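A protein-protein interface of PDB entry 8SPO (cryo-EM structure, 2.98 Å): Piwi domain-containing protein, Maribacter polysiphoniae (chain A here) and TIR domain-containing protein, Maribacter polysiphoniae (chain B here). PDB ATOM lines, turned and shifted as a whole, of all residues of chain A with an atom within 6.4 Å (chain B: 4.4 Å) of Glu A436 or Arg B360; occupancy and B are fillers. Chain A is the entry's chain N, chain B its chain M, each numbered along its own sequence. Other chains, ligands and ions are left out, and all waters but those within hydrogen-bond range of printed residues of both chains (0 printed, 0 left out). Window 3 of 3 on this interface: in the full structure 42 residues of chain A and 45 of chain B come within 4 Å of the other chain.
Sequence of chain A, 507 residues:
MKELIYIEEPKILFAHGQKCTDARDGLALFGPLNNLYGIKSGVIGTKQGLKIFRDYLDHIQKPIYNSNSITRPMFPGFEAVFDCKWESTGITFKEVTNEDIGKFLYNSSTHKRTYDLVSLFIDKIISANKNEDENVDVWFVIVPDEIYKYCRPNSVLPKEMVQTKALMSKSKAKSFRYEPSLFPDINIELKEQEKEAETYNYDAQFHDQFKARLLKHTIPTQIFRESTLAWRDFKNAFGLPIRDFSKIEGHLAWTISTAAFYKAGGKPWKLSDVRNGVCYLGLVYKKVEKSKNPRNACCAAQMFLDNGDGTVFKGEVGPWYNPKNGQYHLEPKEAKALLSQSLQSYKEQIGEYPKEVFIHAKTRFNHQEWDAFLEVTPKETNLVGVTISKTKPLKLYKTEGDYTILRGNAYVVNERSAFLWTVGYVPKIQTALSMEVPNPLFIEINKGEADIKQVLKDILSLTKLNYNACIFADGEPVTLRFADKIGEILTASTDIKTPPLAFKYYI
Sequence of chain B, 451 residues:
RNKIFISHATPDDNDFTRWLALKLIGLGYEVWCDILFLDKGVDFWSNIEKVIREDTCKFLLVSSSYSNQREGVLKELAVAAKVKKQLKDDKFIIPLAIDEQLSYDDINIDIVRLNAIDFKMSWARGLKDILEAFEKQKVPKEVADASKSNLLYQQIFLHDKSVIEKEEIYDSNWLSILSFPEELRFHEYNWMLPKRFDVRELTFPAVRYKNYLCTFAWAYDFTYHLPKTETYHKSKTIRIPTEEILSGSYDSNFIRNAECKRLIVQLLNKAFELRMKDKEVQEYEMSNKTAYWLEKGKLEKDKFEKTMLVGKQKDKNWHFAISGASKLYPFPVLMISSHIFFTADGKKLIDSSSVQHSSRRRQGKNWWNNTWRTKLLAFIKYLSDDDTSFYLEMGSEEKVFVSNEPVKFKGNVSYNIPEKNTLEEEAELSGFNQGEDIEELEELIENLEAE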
ATOM      1  N   LYS A 395       8.962  21.555 -10.541  1.00  0.00           N
ATOM      2  CA  LYS A 395       9.974  21.638  -9.502  1.00  0.00           C
ATOM      3  C   LYS A 395      10.598  23.024  -9.529  1.00  0.00           C
ATOM      4  O   LYS A 395      10.716  23.640 -10.592  1.00  0.00           O
ATOM      5  CB  LYS A 395      11.047  20.566  -9.695  1.00  0.00           C
ATOM      6  CG  LYS A 395      10.577  19.165  -9.340  1.00  0.00           C
ATOM      7  CD  LYS A 395      11.741  18.197  -9.203  1.00  0.00           C
ATOM      8  CE  LYS A 395      11.263  16.761  -9.040  1.00  0.00           C
ATOM      9  NZ  LYS A 395      11.060  16.389  -7.617  1.00  0.00           N
ATOM     10  N   THR A 404      16.630  23.192  -0.105  1.00  0.00           N
ATOM     11  CA  THR A 404      15.465  23.209  -0.974  1.00  0.00           C
ATOM     12  C   THR A 404      14.558  24.399  -0.663  1.00  0.00           C
ATOM     13  O   THR A 404      14.849  25.233   0.199  1.00  0.00           O
ATOM     14  CB  THR A 404      14.697  21.893  -0.852  1.00  0.00           C
ATOM     15  OG1 THR A 404      13.597  21.896  -1.768  1.00  0.00           O
ATOM     16  CG2 THR A 404      14.171  21.697   0.564  1.00  0.00           C
ATOM     17  N   ALA A 432      15.217  19.916   5.746  1.00  0.00           N
ATOM     18  CA  ALA A 432      14.065  19.684   4.890  1.00  0.00           C
ATOM     19  C   ALA A 432      13.457  18.321   5.192  1.00  0.00           C
ATOM     20  O   ALA A 432      14.157  17.383   5.583  1.00  0.00           O
ATOM     21  CB  ALA A 432      14.454  19.761   3.411  1.00  0.00           C
ATOM     22  N   SER A 434      12.245  16.222   3.137  1.00  0.00           N
ATOM     23  CA  SER A 434      12.639  15.250   2.126  1.00  0.00           C
ATOM     24  C   SER A 434      14.151  15.305   1.933  1.00  0.00           C
ATOM     25  O   SER A 434      14.856  16.087   2.574  1.00  0.00           O
ATOM     26  CB  SER A 434      11.912  15.514   0.805  1.00  0.00           C
ATOM     27  OG  SER A 434      12.444  16.649   0.146  1.00  0.00           O
ATOM     28  N   MET A 435      14.651  14.455   1.036  1.00  0.00           N
ATOM     29  CA  MET A 435      16.072  14.411   0.711  1.00  0.00           C
ATOM     30  C   MET A 435      16.376  15.158  -0.582  1.00  0.00           C
ATOM     31  O   MET A 435      17.209  16.069  -0.597  1.00  0.00           O
ATOM     32  CB  MET A 435      16.547  12.957   0.611  1.00  0.00           C
ATOM     33  CG  MET A 435      16.618  12.228   1.942  1.00  0.00           C
ATOM     34  SD  MET A 435      17.246  10.543   1.785  1.00  0.00           S
ATOM     35  CE  MET A 435      18.988  10.848   1.502  1.00  0.00           C
ATOM     36  N   GLU A 436      15.712  14.787  -1.670  1.00  0.00           N
ATOM     37  CA  GLU A 436      15.940  15.411  -2.964  1.00  0.00           C
ATOM     38  C   GLU A 436      14.997  16.604  -3.119  1.00  0.00           C
ATOM     39  O   GLU A 436      14.354  17.044  -2.164  1.00  0.00           O
ATOM     40  CB  GLU A 436      15.764  14.382  -4.079  1.00  0.00           C
ATOM     41  CG  GLU A 436      16.781  13.249  -4.034  1.00  0.00           C
ATOM     42  CD  GLU A 436      16.396  12.081  -4.920  1.00  0.00           C
ATOM     43  OE1 GLU A 436      15.421  12.204  -5.686  1.00  0.00           O
ATOM     44  OE2 GLU A 436      17.072  11.035  -4.845  1.00  0.00           O
ATOM     45  N   VAL A 437      14.911  17.143  -4.330  1.00  0.00           N
ATOM     46  CA  VAL A 437      14.045  18.287  -4.601  1.00  0.00           C
ATOM     47  C   VAL A 437      12.598  17.823  -4.468  1.00  0.00           C
ATOM     48  O   VAL A 437      12.186  16.886  -5.165  1.00  0.00           O
ATOM     49  CB  VAL A 437      14.330  18.877  -5.991  1.00  0.00           C
ATOM     50  CG1 VAL A 437      13.405  20.044  -6.279  1.00  0.00           C
ATOM     51  CG2 VAL A 437      15.787  19.308  -6.088  1.00  0.00           C
ATOM     52  N   PRO A 438      11.794  18.431  -3.598  1.00  0.00           N
ATOM     53  CA  PRO A 438      10.451  17.909  -3.342  1.00  0.00           C
ATOM     54  C   PRO A 438       9.458  18.276  -4.436  1.00  0.00           C
ATOM     55  O   PRO A 438       9.694  19.151  -5.270  1.00  0.00           O
ATOM     56  CB  PRO A 438      10.067  18.569  -2.015  1.00  0.00           C
ATOM     57  CG  PRO A 438      10.800  19.854  -2.023  1.00  0.00           C
ATOM     58  CD  PRO A 438      12.096  19.597  -2.747  1.00  0.00           C
ATOM     59  N   ILE B 340      18.555   9.060 -13.795  1.00  0.00           N
ATOM     60  CA  ILE B 340      19.934   8.584 -13.857  1.00  0.00           C
ATOM     61  C   ILE B 340      19.907   7.124 -14.288  1.00  0.00           C
ATOM     62  O   ILE B 340      19.234   6.300 -13.657  1.00  0.00           O
ATOM     63  CB  ILE B 340      20.674   8.732 -12.516  1.00  0.00           C
ATOM     64  CG1 ILE B 340      20.541  10.155 -11.971  1.00  0.00           C
ATOM     65  CG2 ILE B 340      22.143   8.380 -12.688  1.00  0.00           C
ATOM     66  CD1 ILE B 340      20.947  10.285 -10.524  1.00  0.00           C
ATOM     67  N   PHE B 342      22.369   3.697 -15.890  1.00  0.00           N
ATOM     68  CA  PHE B 342      23.690   3.124 -15.681  1.00  0.00           C
ATOM     69  C   PHE B 342      24.032   2.135 -16.787  1.00  0.00           C
ATOM     70  O   PHE B 342      23.156   1.460 -17.335  1.00  0.00           O
ATOM     71  CB  PHE B 342      23.762   2.425 -14.320  1.00  0.00           C
ATOM     72  CG  PHE B 342      23.477   3.337 -13.166  1.00  0.00           C
ATOM     73  CD1 PHE B 342      22.180   3.540 -12.736  1.00  0.00           C
ATOM     74  CD2 PHE B 342      24.502   3.999 -12.517  1.00  0.00           C
ATOM     75  CE1 PHE B 342      21.911   4.380 -11.680  1.00  0.00           C
ATOM     76  CE2 PHE B 342      24.236   4.841 -11.458  1.00  0.00           C
ATOM     77  CZ  PHE B 342      22.941   5.032 -11.040  1.00  0.00           C
ATOM     78  N   GLN B 356      19.224  -1.347 -11.778  1.00  0.00           N
ATOM     79  CA  GLN B 356      19.095   0.063 -12.128  1.00  0.00           C
ATOM     80  C   GLN B 356      18.437   0.846 -11.001  1.00  0.00           C
ATOM     81  O   GLN B 356      18.896   1.937 -10.640  1.00  0.00           O
ATOM     82  CB  GLN B 356      18.290   0.206 -13.419  1.00  0.00           C
ATOM     83  CG  GLN B 356      18.964  -0.376 -14.653  1.00  0.00           C
ATOM     84  CD  GLN B 356      19.781   0.646 -15.422  1.00  0.00           C
ATOM     85  OE1 GLN B 356      19.713   1.841 -15.154  1.00  0.00           O
ATOM     86  NE2 GLN B 356      20.548   0.174 -16.396  1.00  0.00           N
ATOM     87  N   HIS B 357      17.361   0.305 -10.427  1.00  0.00           N
ATOM     88  CA  HIS B 357      16.652   1.003  -9.361  1.00  0.00           C
ATOM     89  C   HIS B 357      17.546   1.198  -8.142  1.00  0.00           C
ATOM     90  O   HIS B 357      17.611   2.294  -7.574  1.00  0.00           O
ATOM     91  CB  HIS B 357      15.387   0.231  -8.987  1.00  0.00           C
ATOM     92  CG  HIS B 357      14.703   0.749  -7.761  1.00  0.00           C
ATOM     93  ND1 HIS B 357      14.026   1.948  -7.739  1.00  0.00           N
ATOM     94  CD2 HIS B 357      14.589   0.230  -6.517  1.00  0.00           C
ATOM     95  CE1 HIS B 357      13.527   2.148  -6.532  1.00  0.00           C
ATOM     96  NE2 HIS B 357      13.857   1.120  -5.771  1.00  0.00           N
ATOM     97  N   SER B 358      18.250   0.141  -7.727  1.00  0.00           N
ATOM     98  CA  SER B 358      19.120   0.259  -6.561  1.00  0.00           C
ATOM     99  C   SER B 358      20.239   1.263  -6.811  1.00  0.00           C
ATOM    100  O   SER B 358      20.528   2.111  -5.955  1.00  0.00           O
ATOM    101  CB  SER B 358      19.703  -1.106  -6.199  1.00  0.00           C
ATOM    102  OG  SER B 358      18.688  -2.091  -6.120  1.00  0.00           O
ATOM    103  N   SER B 359      20.874   1.192  -7.984  1.00  0.00           N
ATOM    104  CA  SER B 359      21.964   2.110  -8.284  1.00  0.00           C
ATOM    105  C   SER B 359      21.475   3.551  -8.312  1.00  0.00           C
ATOM    106  O   SER B 359      22.156   4.456  -7.814  1.00  0.00           O
ATOM    107  CB  SER B 359      22.612   1.739  -9.616  1.00  0.00           C
ATOM    108  OG  SER B 359      23.126   0.422  -9.576  1.00  0.00           O
ATOM    109  N   ARG B 360      20.300   3.789  -8.894  1.00  0.00           N
ATOM    110  CA  ARG B 360      19.762   5.143  -8.937  1.00  0.00           C
ATOM    111  C   ARG B 360      19.434   5.643  -7.537  1.00  0.00           C
ATOM    112  O   ARG B 360      19.661   6.816  -7.221  1.00  0.00           O
ATOM    113  CB  ARG B 360      18.528   5.182  -9.835  1.00  0.00           C
ATOM    114  CG  ARG B 360      17.988   6.574 -10.103  1.00  0.00           C
ATOM    115  CD  ARG B 360      16.841   6.924  -9.188  1.00  0.00           C
ATOM    116  NE  ARG B 360      16.314   8.255  -9.467  1.00  0.00           N
ATOM    117  CZ  ARG B 360      16.791   9.376  -8.946  1.00  0.00           C
ATOM    118  NH1 ARG B 360      17.810   9.369  -8.102  1.00  0.00           N
ATOM    119  NH2 ARG B 360      16.228  10.533  -9.273  1.00  0.00           N
ATOM    120  N   ARG B 361      18.901   4.768  -6.682  1.00  0.00           N
ATOM    121  CA  ARG B 361      18.600   5.172  -5.316  1.00  0.00           C
ATOM    122  C   ARG B 361      19.867   5.530  -4.552  1.00  0.00           C
ATOM    123  O   ARG B 361      19.869   6.474  -3.754  1.00  0.00           O
ATOM    124  CB  ARG B 361      17.837   4.061  -4.601  1.00  0.00           C
ATOM    125  CG  ARG B 361      16.437   3.875  -5.133  1.00  0.00           C
ATOM    126  CD  ARG B 361      15.502   4.918  -4.555  1.00  0.00           C
ATOM    127  NE  ARG B 361      15.262   6.018  -5.480  1.00  0.00           N
ATOM    128  CZ  ARG B 361      15.037   7.273  -5.114  1.00  0.00           C
ATOM    129  NH1 ARG B 361      15.022   7.635  -3.842  1.00  0.00           N
ATOM    130  NH2 ARG B 361      14.821   8.192  -6.050  1.00  0.00           N
ATOM    131  N   ARG B 362      20.951   4.788  -4.777  1.00  0.00           N
ATOM    132  CA  ARG B 362      22.192   5.090  -4.071  1.00  0.00           C
ATOM    133  C   ARG B 362      22.903   6.312  -4.644  1.00  0.00           C
ATOM    134  O   ARG B 362      23.509   7.082  -3.894  1.00  0.00           O
ATOM    135  CB  ARG B 362      23.124   3.883  -4.100  1.00  0.00           C
ATOM    136  CG  ARG B 362      24.382   4.074  -3.269  1.00  0.00           C
ATOM    137  CD  ARG B 362      25.237   2.823  -3.263  1.00  0.00           C
ATOM    138  NE  ARG B 362      24.570   1.718  -2.583  1.00  0.00           N
ATOM    139  CZ  ARG B 362      24.020   0.672  -3.184  1.00  0.00           C
ATOM    140  NH1 ARG B 362      24.014   0.551  -4.504  1.00  0.00           N
ATOM    141  NH2 ARG B 362      23.456  -0.277  -2.444  1.00  0.00           N
ATOM    142  N   GLN B 363      22.848   6.510  -5.963  1.00  0.00           N
ATOM    143  CA  GLN B 363      23.630   7.584  -6.570  1.00  0.00           C
ATOM    144  C   GLN B 363      23.084   8.956  -6.193  1.00  0.00           C
ATOM    145  O   GLN B 363      23.857   9.885  -5.934  1.00  0.00           O
ATOM    146  CB  GLN B 363      23.665   7.422  -8.090  1.00  0.00           C
ATOM    147  CG  GLN B 363      24.460   8.500  -8.805  1.00  0.00           C
ATOM    148  CD  GLN B 363      25.935   8.472  -8.452  1.00  0.00           C
ATOM    149  OE1 GLN B 363      26.694   7.657  -8.970  1.00  0.00           O
ATOM    150  NE2 GLN B 363      26.347   9.365  -7.561  1.00  0.00           N
ATOM    151  N   GLY B 364      21.765   9.107  -6.158  1.00  0.00           N
ATOM    152  CA  GLY B 364      21.166  10.373  -5.792  1.00  0.00           C
ATOM    153  C   GLY B 364      21.190  10.683  -4.318  1.00  0.00           C
ATOM    154  O   GLY B 364      20.687  11.730  -3.899  1.00  0.00           O
ATOM    155  N   TRP B 372      21.221  18.777  -9.034  1.00  0.00           N
ATOM    156  CA  TRP B 372      20.170  18.528 -10.014  1.00  0.00           C
ATOM    157  C   TRP B 372      19.936  19.757 -10.881  1.00  0.00           C
ATOM    158  O   TRP B 372      19.758  19.648 -12.100  1.00  0.00           O
ATOM    159  CB  TRP B 372      18.867  18.128  -9.316  1.00  0.00           C
ATOM    160  CG  TRP B 372      18.945  16.901  -8.459  1.00  0.00           C
ATOM    161  CD1 TRP B 372      19.106  16.860  -7.107  1.00  0.00           C
ATOM    162  CD2 TRP B 372      18.835  15.536  -8.888  1.00  0.00           C
ATOM    163  NE1 TRP B 372      19.117  15.560  -6.667  1.00  0.00           N
ATOM    164  CE2 TRP B 372      18.954  14.727  -7.740  1.00  0.00           C
ATOM    165  CE3 TRP B 372      18.655  14.920 -10.130  1.00  0.00           C
ATOM    166  CZ2 TRP B 372      18.898  13.339  -7.800  1.00  0.00           C
ATOM    167  CZ3 TRP B 372      18.601  13.541 -10.185  1.00  0.00           C
ATOM    168  CH2 TRP B 372      18.722  12.767  -9.027  1.00  0.00           C
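OG of Ser A434 is in hydrogen-bond range of O of Glu A436, at 3.0 Å.
Ala A432 touches none of the printed residues of chain B. Printed residues of chain B within 4 Å of Glu A436: Arg B360, Arg B361 and Gly B364. Pro A438 touches none of the printed residues of chain B. Arg B360 touches just one residue of chain A: Glu A436. Printed residues of chain A within 4 Å of Arg B361: Glu A436. Printed residues of chain A within 4 Å of Gly B364: Glu A436 (3.8 Å). The nearest printed residue of chain A that does not touch Gly B364 is Met A435 (5.7 Å).
Of the 8 printed residues of chain A, 1 touches a printed residue of chain B. Of the 12 printed residues of chain B, 3 touch a printed residue of chain A. Printed residues of chain B that touch a printed residue of chain A: Arg B360, Arg B361 and Gly B364.
OE2 of Glu A436 touches O of Gly B364 (3.8 Å).
The guanidinium group (NH1) of Arg B360 lies within salt-bridge range of the side-chain carboxylate (OE2) of Glu A436. The guanidinium group (NH2) of Arg B361 is in salt-bridge range of the side-chain carboxylate (OE2) of Glu A436 (3.8 Å).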
